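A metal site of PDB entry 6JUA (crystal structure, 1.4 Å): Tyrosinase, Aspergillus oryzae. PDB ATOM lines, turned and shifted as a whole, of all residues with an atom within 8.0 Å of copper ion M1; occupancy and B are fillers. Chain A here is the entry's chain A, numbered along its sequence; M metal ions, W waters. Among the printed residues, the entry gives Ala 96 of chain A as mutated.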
ATOM      1  N   HIS A  71      19.616 -34.034   3.953  1.00  0.00           N
ATOM      2  CA  HIS A  71      19.155 -32.803   3.337  1.00  0.00           C
ATOM      3  C   HIS A  71      17.651 -32.722   3.157  1.00  0.00           C
ATOM      4  O   HIS A  71      17.061 -31.652   3.371  1.00  0.00           O
ATOM      5  CB  HIS A  71      19.842 -32.664   1.964  1.00  0.00           C
ATOM      6  CG  HIS A  71      19.666 -31.337   1.303  1.00  0.00           C
ATOM      7  ND1 HIS A  71      18.848 -31.137   0.222  1.00  0.00           N
ATOM      8  CD2 HIS A  71      20.198 -30.119   1.563  1.00  0.00           C
ATOM      9  CE1 HIS A  71      18.873 -29.876  -0.161  1.00  0.00           C
ATOM     10  NE2 HIS A  71      19.695 -29.236   0.644  1.00  0.00           N
ATOM     11  N   GLY A  72      16.997 -33.828   2.789  1.00  0.00           N
ATOM     12  CA  GLY A  72      15.583 -33.853   2.437  1.00  0.00           C
ATOM     13  C   GLY A  72      14.934 -35.209   2.584  1.00  0.00           C
ATOM     14  O   GLY A  72      14.960 -35.793   3.676  1.00  0.00           O
ATOM     15  N   PHE A  95      16.242 -31.439   7.510  1.00  0.00           N
ATOM     16  CA  PHE A  95      17.160 -30.699   8.360  1.00  0.00           C
ATOM     17  C   PHE A  95      17.681 -29.439   7.668  1.00  0.00           C
ATOM     18  O   PHE A  95      18.027 -28.443   8.294  1.00  0.00           O
ATOM     19  CB  PHE A  95      18.346 -31.595   8.741  1.00  0.00           C
ATOM     20  CG  PHE A  95      18.015 -32.668   9.745  1.00  0.00           C
ATOM     21  CD1 PHE A  95      17.583 -32.346  11.027  1.00  0.00           C
ATOM     22  CD2 PHE A  95      18.154 -34.008   9.400  1.00  0.00           C
ATOM     23  CE1 PHE A  95      17.275 -33.347  11.929  1.00  0.00           C
ATOM     24  CE2 PHE A  95      17.838 -35.014  10.300  1.00  0.00           C
ATOM     25  CZ  PHE A  95      17.419 -34.671  11.569  1.00  0.00           C
ATOM     26  N   ALA A  96      17.797 -29.496   6.346  1.00  0.00           N
ATOM     27  CA  ALA A  96      18.443 -28.418   5.606  1.00  0.00           C
ATOM     28  C   ALA A  96      17.734 -27.088   5.833  1.00  0.00           C
ATOM     29  O   ALA A  96      16.493 -27.038   5.930  1.00  0.00           O
ATOM     30  CB  ALA A  96      18.466 -28.768   4.125  1.00  0.00           C
ATOM     31  N   VAL A  97      18.525 -26.017   5.932  1.00  0.00           N
ATOM     32  CA  VAL A  97      18.023 -24.653   6.041  1.00  0.00           C
ATOM     33  C   VAL A  97      18.005 -23.972   4.671  1.00  0.00           C
ATOM     34  O   VAL A  97      19.068 -23.786   4.075  1.00  0.00           O
ATOM     35  CB  VAL A  97      18.838 -23.769   7.005  1.00  0.00           C
ATOM     36  CG1 VAL A  97      18.352 -22.331   7.039  1.00  0.00           C
ATOM     37  CG2 VAL A  97      18.807 -24.364   8.406  1.00  0.00           C
ATOM     38  N   HIS A  98      16.799 -23.609   4.273  1.00  0.00           N
ATOM     39  CA  HIS A  98      16.562 -22.789   3.076  1.00  0.00           C
ATOM     40  C   HIS A  98      15.714 -21.576   3.402  1.00  0.00           C
ATOM     41  O   HIS A  98      14.881 -21.619   4.310  1.00  0.00           O
ATOM     42  CB  HIS A  98      15.928 -23.654   1.989  1.00  0.00           C
ATOM     43  CG  HIS A  98      16.741 -24.861   1.639  1.00  0.00           C
ATOM     44  ND1 HIS A  98      16.241 -26.143   1.767  1.00  0.00           N
ATOM     45  CD2 HIS A  98      18.009 -25.007   1.184  1.00  0.00           C
ATOM     46  CE1 HIS A  98      17.159 -27.011   1.386  1.00  0.00           C
ATOM     47  NE2 HIS A  98      18.250 -26.359   1.027  1.00  0.00           N
ATOM     48  N   PHE A 103      21.325 -20.295   5.944  1.00  0.00           N
ATOM     49  CA  PHE A 103      21.579 -21.103   4.746  1.00  0.00           C
ATOM     50  C   PHE A 103      23.061 -21.338   4.515  1.00  0.00           C
ATOM     51  O   PHE A 103      23.451 -22.508   4.301  1.00  0.00           O
ATOM     52  CB  PHE A 103      20.897 -20.483   3.523  1.00  0.00           C
ATOM     53  CG  PHE A 103      21.424 -20.978   2.193  1.00  0.00           C
ATOM     54  CD1 PHE A 103      21.036 -22.198   1.648  1.00  0.00           C
ATOM     55  CD2 PHE A 103      22.319 -20.202   1.472  1.00  0.00           C
ATOM     56  CE1 PHE A 103      21.543 -22.603   0.430  1.00  0.00           C
ATOM     57  CE2 PHE A 103      22.852 -20.614   0.268  1.00  0.00           C
ATOM     58  CZ  PHE A 103      22.461 -21.838  -0.255  1.00  0.00           C
ATOM     59  N   TRP A 106      24.678 -23.567   7.670  1.00  0.00           N
ATOM     60  CA  TRP A 106      24.220 -24.954   7.744  1.00  0.00           C
ATOM     61  C   TRP A 106      24.913 -25.799   6.686  1.00  0.00           C
ATOM     62  O   TRP A 106      25.398 -26.910   6.939  1.00  0.00           O
ATOM     63  CB  TRP A 106      22.687 -25.048   7.602  1.00  0.00           C
ATOM     64  CG  TRP A 106      22.204 -26.456   7.862  1.00  0.00           C
ATOM     65  CD1 TRP A 106      21.791 -26.988   9.055  1.00  0.00           C
ATOM     66  CD2 TRP A 106      22.079 -27.521   6.903  1.00  0.00           C
ATOM     67  NE1 TRP A 106      21.422 -28.306   8.890  1.00  0.00           N
ATOM     68  CE2 TRP A 106      21.596 -28.650   7.587  1.00  0.00           C
ATOM     69  CE3 TRP A 106      22.348 -27.616   5.537  1.00  0.00           C
ATOM     70  CZ2 TRP A 106      21.365 -29.877   6.944  1.00  0.00           C
ATOM     71  CZ3 TRP A 106      22.124 -28.814   4.886  1.00  0.00           C
ATOM     72  CH2 TRP A 106      21.636 -29.925   5.596  1.00  0.00           C
ATOM     73  N   HIS A 107      24.983 -25.247   5.468  1.00  0.00           N
ATOM     74  CA  HIS A 107      25.606 -25.962   4.351  1.00  0.00           C
ATOM     75  C   HIS A 107      27.120 -26.011   4.501  1.00  0.00           C
ATOM     76  O   HIS A 107      27.755 -26.974   4.032  1.00  0.00           O
ATOM     77  CB  HIS A 107      25.130 -25.383   3.010  1.00  0.00           C
ATOM     78  CG  HIS A 107      23.709 -25.697   2.652  1.00  0.00           C
ATOM     79  ND1 HIS A 107      22.648 -24.952   3.116  1.00  0.00           N
ATOM     80  CD2 HIS A 107      23.155 -26.686   1.904  1.00  0.00           C
ATOM     81  CE1 HIS A 107      21.507 -25.451   2.664  1.00  0.00           C
ATOM     82  NE2 HIS A 107      21.787 -26.503   1.919  1.00  0.00           N
ATOM     83  N   TYR A 110      27.623 -29.072   6.521  1.00  0.00           N
ATOM     84  CA  TYR A 110      27.223 -30.259   5.757  1.00  0.00           C
ATOM     85  C   TYR A 110      28.303 -30.671   4.755  1.00  0.00           C
ATOM     86  O   TYR A 110      28.604 -31.854   4.599  1.00  0.00           O
ATOM     87  CB  TYR A 110      25.937 -29.955   4.999  1.00  0.00           C
ATOM     88  CG  TYR A 110      25.142 -31.093   4.421  1.00  0.00           C
ATOM     89  CD1 TYR A 110      25.086 -32.362   4.986  1.00  0.00           C
ATOM     90  CD2 TYR A 110      24.420 -30.861   3.244  1.00  0.00           C
ATOM     91  CE1 TYR A 110      24.333 -33.376   4.409  1.00  0.00           C
ATOM     92  CE2 TYR A 110      23.663 -31.850   2.671  1.00  0.00           C
ATOM     93  CZ  TYR A 110      23.620 -33.108   3.253  1.00  0.00           C
ATOM     94  OH  TYR A 110      22.851 -34.060   2.622  1.00  0.00           O
ATOM     95  N   GLU A 329      22.023 -17.222  -2.122  1.00  0.00           N
ATOM     96  CA  GLU A 329      21.067 -18.339  -2.216  1.00  0.00           C
ATOM     97  C   GLU A 329      20.302 -18.316  -3.532  1.00  0.00           C
ATOM     98  O   GLU A 329      20.085 -19.362  -4.158  1.00  0.00           O
ATOM     99  CB  GLU A 329      20.108 -18.294  -1.018  1.00  0.00           C
ATOM    100  CG  GLU A 329      19.184 -19.500  -0.934  1.00  0.00           C
ATOM    101  CD  GLU A 329      18.368 -19.554   0.339  1.00  0.00           C
ATOM    102  OE1 GLU A 329      18.353 -18.567   1.107  1.00  0.00           O
ATOM    103  OE2 GLU A 329      17.724 -20.621   0.565  1.00  0.00           O
ATOM    104  N   HIS A 332      22.546 -19.665  -6.188  1.00  0.00           N
ATOM    105  CA  HIS A 332      22.589 -21.108  -5.926  1.00  0.00           C
ATOM    106  C   HIS A 332      21.337 -21.839  -6.409  1.00  0.00           C
ATOM    107  O   HIS A 332      21.412 -22.984  -6.869  1.00  0.00           O
ATOM    108  CB  HIS A 332      22.854 -21.330  -4.429  1.00  0.00           C
ATOM    109  CG  HIS A 332      22.120 -22.448  -3.782  1.00  0.00           C
ATOM    110  ND1 HIS A 332      20.816 -22.335  -3.341  1.00  0.00           N
ATOM    111  CD2 HIS A 332      22.492 -23.709  -3.458  1.00  0.00           C
ATOM    112  CE1 HIS A 332      20.415 -23.474  -2.788  1.00  0.00           C
ATOM    113  NE2 HIS A 332      21.421 -24.322  -2.848  1.00  0.00           N
ATOM    114  N   ASN A 333      20.186 -21.187  -6.326  1.00  0.00           N
ATOM    115  CA  ASN A 333      18.901 -21.754  -6.744  1.00  0.00           C
ATOM    116  C   ASN A 333      18.852 -21.927  -8.253  1.00  0.00           C
ATOM    117  O   ASN A 333      18.395 -22.963  -8.737  1.00  0.00           O
ATOM    118  CB  ASN A 333      17.737 -20.857  -6.305  1.00  0.00           C
ATOM    119  CG  ASN A 333      17.409 -20.912  -4.831  1.00  0.00           C
ATOM    120  OD1 ASN A 333      17.970 -21.688  -4.060  1.00  0.00           O
ATOM    121  ND2 ASN A 333      16.463 -20.068  -4.411  1.00  0.00           N
ATOM    122  N   HIS A 336      20.997 -24.944  -9.322  1.00  0.00           N
ATOM    123  CA  HIS A 336      20.291 -26.198  -9.096  1.00  0.00           C
ATOM    124  C   HIS A 336      19.400 -26.528 -10.290  1.00  0.00           C
ATOM    125  O   HIS A 336      19.435 -27.641 -10.829  1.00  0.00           O
ATOM    126  CB  HIS A 336      19.472 -26.123  -7.798  1.00  0.00           C
ATOM    127  CG  HIS A 336      20.162 -26.574  -6.552  1.00  0.00           C
ATOM    128  ND1 HIS A 336      20.392 -27.902  -6.266  1.00  0.00           N
ATOM    129  CD2 HIS A 336      20.645 -25.906  -5.465  1.00  0.00           C
ATOM    130  CE1 HIS A 336      20.990 -28.032  -5.093  1.00  0.00           C
ATOM    131  NE2 HIS A 336      21.163 -26.821  -4.582  1.00  0.00           N
ATOM    132  N   VAL A 363      14.452 -29.891  -4.270  1.00  0.00           N
ATOM    133  CA  VAL A 363      14.984 -29.864  -2.908  1.00  0.00           C
ATOM    134  C   VAL A 363      14.977 -31.229  -2.234  1.00  0.00           C
ATOM    135  O   VAL A 363      15.989 -31.633  -1.641  1.00  0.00           O
ATOM    136  CB  VAL A 363      14.209 -28.874  -2.016  1.00  0.00           C
ATOM    137  CG1 VAL A 363      14.693 -28.948  -0.578  1.00  0.00           C
ATOM    138  CG2 VAL A 363      14.369 -27.467  -2.574  1.00  0.00           C
ATOM    139  N   ALA A 366      17.841 -33.433  -4.278  1.00  0.00           N
ATOM    140  CA  ALA A 366      19.016 -32.916  -4.985  1.00  0.00           C
ATOM    141  C   ALA A 366      20.329 -33.461  -4.426  1.00  0.00           C
ATOM    142  O   ALA A 366      21.297 -33.640  -5.191  1.00  0.00           O
ATOM    143  CB  ALA A 366      19.033 -31.393  -5.025  1.00  0.00           C
ATOM    144  N   ALA A 367      20.398 -33.740  -3.144  1.00  0.00           N
ATOM    145  CA  ALA A 367      21.647 -34.141  -2.489  1.00  0.00           C
ATOM    146  C   ALA A 367      22.147 -35.495  -2.967  1.00  0.00           C
ATOM    147  O   ALA A 367      23.334 -35.835  -2.781  1.00  0.00           O
ATOM    148  CB  ALA A 367      21.498 -34.133  -0.974  1.00  0.00           C
ATOM    149  N   PHE A 372      25.994 -32.226  -6.384  1.00  0.00           N
ATOM    150  CA  PHE A 372      25.455 -31.409  -5.290  1.00  0.00           C
ATOM    151  C   PHE A 372      26.570 -30.878  -4.400  1.00  0.00           C
ATOM    152  O   PHE A 372      26.601 -29.706  -4.018  1.00  0.00           O
ATOM    153  CB  PHE A 372      24.443 -32.221  -4.471  1.00  0.00           C
ATOM    154  CG  PHE A 372      23.941 -31.530  -3.225  1.00  0.00           C
ATOM    155  CD1 PHE A 372      24.637 -31.579  -2.020  1.00  0.00           C
ATOM    156  CD2 PHE A 372      22.768 -30.809  -3.250  1.00  0.00           C
ATOM    157  CE1 PHE A 372      24.171 -30.945  -0.892  1.00  0.00           C
ATOM    158  CE2 PHE A 372      22.266 -30.177  -2.116  1.00  0.00           C
ATOM    159  CZ  PHE A 372      22.981 -30.233  -0.920  1.00  0.00           C
ATOM    160  N   HIS A 376      27.856 -27.079  -3.728  1.00  0.00           N
ATOM    161  CA  HIS A 376      27.927 -26.484  -2.398  1.00  0.00           C
ATOM    162  C   HIS A 376      29.342 -26.192  -1.943  1.00  0.00           C
ATOM    163  O   HIS A 376      29.542 -25.276  -1.120  1.00  0.00           O
ATOM    164  CB  HIS A 376      27.145 -27.360  -1.389  1.00  0.00           C
ATOM    165  CG  HIS A 376      25.716 -26.885  -1.400  1.00  0.00           C
ATOM    166  ND1 HIS A 376      25.297 -25.767  -0.705  1.00  0.00           N
ATOM    167  CD2 HIS A 376      24.657 -27.365  -2.075  1.00  0.00           C
ATOM    168  CE1 HIS A 376      24.011 -25.591  -0.953  1.00  0.00           C
ATOM    169  NE2 HIS A 376      23.596 -26.548  -1.770  1.00  0.00           N
ATOM    170  N   PHE A 517      13.413 -22.742  -5.825  1.00  0.00           N
ATOM    171  CA  PHE A 517      13.960 -23.998  -5.316  1.00  0.00           C
ATOM    172  C   PHE A 517      13.197 -24.399  -4.050  1.00  0.00           C
ATOM    173  O   PHE A 517      13.596 -24.043  -2.943  1.00  0.00           O
ATOM    174  CB  PHE A 517      15.460 -23.878  -5.089  1.00  0.00           C
ATOM    175  CG  PHE A 517      16.217 -25.144  -4.751  1.00  0.00           C
ATOM    176  CD1 PHE A 517      16.208 -26.271  -5.557  1.00  0.00           C
ATOM    177  CD2 PHE A 517      16.956 -25.215  -3.569  1.00  0.00           C
ATOM    178  CE1 PHE A 517      16.887 -27.420  -5.199  1.00  0.00           C
ATOM    179  CE2 PHE A 517      17.661 -26.331  -3.207  1.00  0.00           C
ATOM    180  CZ  PHE A 517      17.640 -27.452  -4.031  1.00  0.00           C
HETATM  181 CU    CU M   1      20.154 -27.277   0.614  1.00  0.00          CU
HETATM  182 CU    CU M   2      21.543 -26.251  -2.640  1.00  0.00          CU
HETATM  183  O   HOH W   1      20.695 -27.199  -1.495  1.00  0.00           O
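The backbone carbonyl oxygen of Val 363 sits at hydrogen-bond distance from a ring nitrogen (ND1) of His 71 (3.4 Å).
The backbone carbonyl oxygen (O) of Phe 103 lies within hydrogen-bond range of a ring nitrogen (ND1) of His 107, at 2.8 Å.
The side-chain hydroxyl of Tyr 110 sits close to the backbone NH of His 71 (3.5 Å).
Within 4 Å of copper ion M1: His 71, His 98 and His 107.
The nearest printed residue that does not touch copper ion M1 is Ala 96 (4.2 Å).
Copper ion M1 is bound by NE2 of His 71, NE2 of His 98, water W1 and NE2 of His 107.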
